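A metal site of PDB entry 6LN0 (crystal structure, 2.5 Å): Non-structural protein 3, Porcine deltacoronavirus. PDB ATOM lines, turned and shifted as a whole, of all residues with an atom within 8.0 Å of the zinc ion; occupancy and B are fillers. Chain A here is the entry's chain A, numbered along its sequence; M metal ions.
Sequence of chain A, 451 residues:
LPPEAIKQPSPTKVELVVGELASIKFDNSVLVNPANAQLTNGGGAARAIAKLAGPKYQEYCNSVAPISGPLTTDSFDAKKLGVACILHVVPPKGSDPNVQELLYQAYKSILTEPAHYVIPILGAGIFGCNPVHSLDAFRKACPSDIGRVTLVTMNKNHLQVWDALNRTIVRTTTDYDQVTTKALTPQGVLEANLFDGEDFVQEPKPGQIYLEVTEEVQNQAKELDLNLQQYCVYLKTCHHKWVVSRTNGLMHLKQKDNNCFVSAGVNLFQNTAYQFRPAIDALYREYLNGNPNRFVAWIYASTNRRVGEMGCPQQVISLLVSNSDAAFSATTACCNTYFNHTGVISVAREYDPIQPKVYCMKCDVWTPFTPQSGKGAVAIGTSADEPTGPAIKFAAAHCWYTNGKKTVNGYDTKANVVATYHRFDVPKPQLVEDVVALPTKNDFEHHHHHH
The side-chain sulfur of Cys 334 lies close to the side-chain hydroxyl of Thr 332 (3.7 Å).
The backbone NH of Cys 334 lies within hydrogen-bond range of the side-chain hydroxyl of Thr 367 (3.3 Å).
OG1 of Thr 332 lies within hydrogen-bond range of N of Cys 335, at 3.4 Å.
The side-chain sulfur of Cys 335 lies close to the side-chain hydroxyl of Thr 337 (3.3 Å).
The side-chain sulfur (SG) of Cys 360 sits close to the backbone NH (N) of Lys 362, 3.5 Å away.
N of Cys 360 is in hydrogen-bond range of O of Val 365 (3.0 Å).
The backbone NH of Thr 332 is in hydrogen-bond range of the backbone carbonyl oxygen of Thr 337 (3.0 Å).
N of Asn 336 sits at hydrogen-bond distance from OG1 of Thr 332, 3.2 Å away.
Thr 332 touches the zinc ion.
The side-chain sulfur (SG) of Cys 334 is bound to the zinc ion, at 2.3 Å.
The zinc ion is bound by the side-chain sulfur (SG) of Cys 335.
SG of Cys 360 binds the zinc ion, at 2.3 Å.
SG of Cys 363 is bound to the zinc ion, 2.3 Å away.
The zinc ion has four donor atoms within binding distance.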
ATOM      1  N   THR A 332      -1.119   3.577 -16.919  1.00  0.00           N
ATOM      2  CA  THR A 332      -1.019   2.725 -15.741  1.00  0.00           C
ATOM      3  C   THR A 332      -1.126   1.254 -16.127  1.00  0.00           C
ATOM      4  O   THR A 332      -1.710   0.895 -17.148  1.00  0.00           O
ATOM      5  CB  THR A 332      -2.100   3.100 -14.716  1.00  0.00           C
ATOM      6  OG1 THR A 332      -3.396   3.028 -15.315  1.00  0.00           O
ATOM      7  CG2 THR A 332      -1.885   4.523 -14.200  1.00  0.00           C
ATOM      8  N   ALA A 333      -0.526   0.405 -15.315  1.00  0.00           N
ATOM      9  CA  ALA A 333      -0.689  -1.036 -15.488  1.00  0.00           C
ATOM     10  C   ALA A 333      -2.033  -1.503 -14.955  1.00  0.00           C
ATOM     11  O   ALA A 333      -2.614  -2.457 -15.480  1.00  0.00           O
ATOM     12  CB  ALA A 333       0.444  -1.790 -14.809  1.00  0.00           C
ATOM     13  N   CYS A 334      -2.571  -0.818 -13.951  1.00  0.00           N
ATOM     14  CA  CYS A 334      -3.822  -1.262 -13.349  1.00  0.00           C
ATOM     15  C   CYS A 334      -5.012  -1.034 -14.284  1.00  0.00           C
ATOM     16  O   CYS A 334      -5.852  -1.929 -14.440  1.00  0.00           O
ATOM     17  CB  CYS A 334      -4.038  -0.544 -12.023  1.00  0.00           C
ATOM     18  SG  CYS A 334      -3.736   1.203 -12.143  1.00  0.00           S
ATOM     19  N   CYS A 335      -5.118   0.140 -14.915  1.00  0.00           N
ATOM     20  CA  CYS A 335      -6.292   0.387 -15.749  1.00  0.00           C
ATOM     21  C   CYS A 335      -5.992   1.049 -17.085  1.00  0.00           C
ATOM     22  O   CYS A 335      -6.939   1.471 -17.765  1.00  0.00           O
ATOM     23  CB  CYS A 335      -7.307   1.250 -14.975  1.00  0.00           C
ATOM     24  SG  CYS A 335      -6.671   2.760 -14.216  1.00  0.00           S
ATOM     25  N   ASN A 336      -4.739   1.135 -17.506  1.00  0.00           N
ATOM     26  CA  ASN A 336      -4.361   1.801 -18.774  1.00  0.00           C
ATOM     27  C   ASN A 336      -4.964   3.199 -18.897  1.00  0.00           C
ATOM     28  O   ASN A 336      -5.550   3.588 -19.923  1.00  0.00           O
ATOM     29  CB  ASN A 336      -4.733   0.909 -19.952  1.00  0.00           C
ATOM     30  CG  ASN A 336      -4.036  -0.430 -19.849  1.00  0.00           C
ATOM     31  OD1 ASN A 336      -4.605  -1.401 -19.333  1.00  0.00           O
ATOM     32  ND2 ASN A 336      -2.778  -0.495 -20.286  1.00  0.00           N
ATOM     33  N   THR A 337      -4.822   3.978 -17.835  1.00  0.00           N
ATOM     34  CA  THR A 337      -5.117   5.408 -17.885  1.00  0.00           C
ATOM     35  C   THR A 337      -3.857   6.174 -18.293  1.00  0.00           C
ATOM     36  O   THR A 337      -2.761   5.857 -17.825  1.00  0.00           O
ATOM     37  CB  THR A 337      -5.645   5.866 -16.542  1.00  0.00           C
ATOM     38  OG1 THR A 337      -6.922   5.238 -16.323  1.00  0.00           O
ATOM     39  CG2 THR A 337      -5.821   7.406 -16.499  1.00  0.00           C
ATOM     40  N   VAL A 358       3.293   4.909  -9.646  1.00  0.00           N
ATOM     41  CA  VAL A 358       2.489   6.079  -9.341  1.00  0.00           C
ATOM     42  C   VAL A 358       1.207   5.630  -8.683  1.00  0.00           C
ATOM     43  O   VAL A 358       0.829   4.451  -8.721  1.00  0.00           O
ATOM     44  CB  VAL A 358       2.170   6.942 -10.580  1.00  0.00           C
ATOM     45  CG1 VAL A 358       3.428   7.628 -11.073  1.00  0.00           C
ATOM     46  CG2 VAL A 358       1.505   6.093 -11.698  1.00  0.00           C
ATOM     47  N   TYR A 359       0.527   6.581  -8.085  1.00  0.00           N
ATOM     48  CA  TYR A 359      -0.756   6.333  -7.438  1.00  0.00           C
ATOM     49  C   TYR A 359      -1.871   6.497  -8.454  1.00  0.00           C
ATOM     50  O   TYR A 359      -2.012   7.561  -9.071  1.00  0.00           O
ATOM     51  CB  TYR A 359      -0.960   7.290  -6.275  1.00  0.00           C
ATOM     52  CG  TYR A 359      -2.267   7.057  -5.575  1.00  0.00           C
ATOM     53  CD1 TYR A 359      -2.483   5.912  -4.817  1.00  0.00           C
ATOM     54  CD2 TYR A 359      -3.296   7.956  -5.702  1.00  0.00           C
ATOM     55  CE1 TYR A 359      -3.680   5.701  -4.187  1.00  0.00           C
ATOM     56  CE2 TYR A 359      -4.509   7.748  -5.067  1.00  0.00           C
ATOM     57  CZ  TYR A 359      -4.686   6.618  -4.306  1.00  0.00           C
ATOM     58  OH  TYR A 359      -5.896   6.381  -3.666  1.00  0.00           O
ATOM     59  N   CYS A 360      -2.672   5.460  -8.617  1.00  0.00           N
ATOM     60  CA  CYS A 360      -3.863   5.552  -9.456  1.00  0.00           C
ATOM     61  C   CYS A 360      -5.053   5.897  -8.565  1.00  0.00           C
ATOM     62  O   CYS A 360      -5.434   5.108  -7.692  1.00  0.00           O
ATOM     63  CB  CYS A 360      -4.133   4.232 -10.187  1.00  0.00           C
ATOM     64  SG  CYS A 360      -5.657   4.354 -11.200  1.00  0.00           S
ATOM     65  N   MET A 361      -5.650   7.058  -8.813  1.00  0.00           N
ATOM     66  CA  MET A 361      -6.823   7.458  -8.027  1.00  0.00           C
ATOM     67  C   MET A 361      -8.021   6.596  -8.341  1.00  0.00           C
ATOM     68  O   MET A 361      -8.826   6.304  -7.445  1.00  0.00           O
ATOM     69  CB  MET A 361      -7.153   8.935  -8.267  1.00  0.00           C
ATOM     70  CG  MET A 361      -6.972   9.407  -9.683  1.00  0.00           C
ATOM     71  SD  MET A 361      -6.653  11.209  -9.811  1.00  0.00           S
ATOM     72  CE  MET A 361      -5.366  11.478  -8.599  1.00  0.00           C
ATOM     73  N   LYS A 362      -8.148   6.129  -9.586  1.00  0.00           N
ATOM     74  CA  LYS A 362      -9.299   5.336  -9.975  1.00  0.00           C
ATOM     75  C   LYS A 362      -9.381   4.031  -9.186  1.00  0.00           C
ATOM     76  O   LYS A 362     -10.406   3.730  -8.572  1.00  0.00           O
ATOM     77  CB  LYS A 362      -9.267   5.055 -11.474  1.00  0.00           C
ATOM     78  CG  LYS A 362      -9.435   6.312 -12.334  1.00  0.00           C
ATOM     79  CD  LYS A 362      -9.328   5.988 -13.809  1.00  0.00           C
ATOM     80  CE  LYS A 362      -9.384   7.249 -14.665  1.00  0.00           C
ATOM     81  NZ  LYS A 362      -9.304   6.914 -16.124  1.00  0.00           N
ATOM     82  N   CYS A 363      -8.293   3.239  -9.189  1.00  0.00           N
ATOM     83  CA  CYS A 363      -8.243   1.917  -8.575  1.00  0.00           C
ATOM     84  C   CYS A 363      -7.702   1.918  -7.150  1.00  0.00           C
ATOM     85  O   CYS A 363      -7.696   0.867  -6.504  1.00  0.00           O
ATOM     86  CB  CYS A 363      -7.348   0.976  -9.400  1.00  0.00           C
ATOM     87  SG  CYS A 363      -7.464   1.042 -11.208  1.00  0.00           S
ATOM     88  N   ASP A 364      -7.177   3.050  -6.686  1.00  0.00           N
ATOM     89  CA  ASP A 364      -6.622   3.169  -5.346  1.00  0.00           C
ATOM     90  C   ASP A 364      -5.549   2.109  -5.089  1.00  0.00           C
ATOM     91  O   ASP A 364      -5.648   1.308  -4.170  1.00  0.00           O
ATOM     92  CB  ASP A 364      -7.711   3.098  -4.286  1.00  0.00           C
ATOM     93  CG  ASP A 364      -7.179   3.367  -2.891  1.00  0.00           C
ATOM     94  OD1 ASP A 364      -6.157   4.093  -2.784  1.00  0.00           O
ATOM     95  OD2 ASP A 364      -7.770   2.856  -1.918  1.00  0.00           O
ATOM     96  N   VAL A 365      -4.501   2.149  -5.921  1.00  0.00           N
ATOM     97  CA  VAL A 365      -3.331   1.290  -5.768  1.00  0.00           C
ATOM     98  C   VAL A 365      -2.106   2.046  -6.265  1.00  0.00           C
ATOM     99  O   VAL A 365      -2.207   2.960  -7.092  1.00  0.00           O
ATOM    100  CB  VAL A 365      -3.443  -0.037  -6.557  1.00  0.00           C
ATOM    101  CG1 VAL A 365      -4.415  -0.968  -5.887  1.00  0.00           C
ATOM    102  CG2 VAL A 365      -3.877   0.239  -7.977  1.00  0.00           C
ATOM    103  N   THR A 367       0.701   1.597  -8.668  1.00  0.00           N
ATOM    104  CA  THR A 367       0.798   0.789  -9.867  1.00  0.00           C
ATOM    105  C   THR A 367       2.077   1.067 -10.634  1.00  0.00           C
ATOM    106  O   THR A 367       2.568   2.194 -10.640  1.00  0.00           O
ATOM    107  CB  THR A 367      -0.383   1.072 -10.797  1.00  0.00           C
ATOM    108  OG1 THR A 367      -0.228   0.312 -11.990  1.00  0.00           O
ATOM    109  CG2 THR A 367      -0.430   2.563 -11.169  1.00  0.00           C
ATOM    110  N   PRO A 368       2.641   0.053 -11.298  1.00  0.00           N
ATOM    111  CA  PRO A 368       3.664   0.333 -12.314  1.00  0.00           C
ATOM    112  C   PRO A 368       3.038   0.965 -13.552  1.00  0.00           C
ATOM    113  O   PRO A 368       1.811   1.083 -13.655  1.00  0.00           O
ATOM    114  CB  PRO A 368       4.254  -1.055 -12.619  1.00  0.00           C
ATOM    115  CG  PRO A 368       3.839  -1.901 -11.468  1.00  0.00           C
ATOM    116  CD  PRO A 368       2.492  -1.397 -11.060  1.00  0.00           C
HETATM  117 ZN    ZN M   1      -5.738   2.262 -12.209  1.00  0.00          ZN
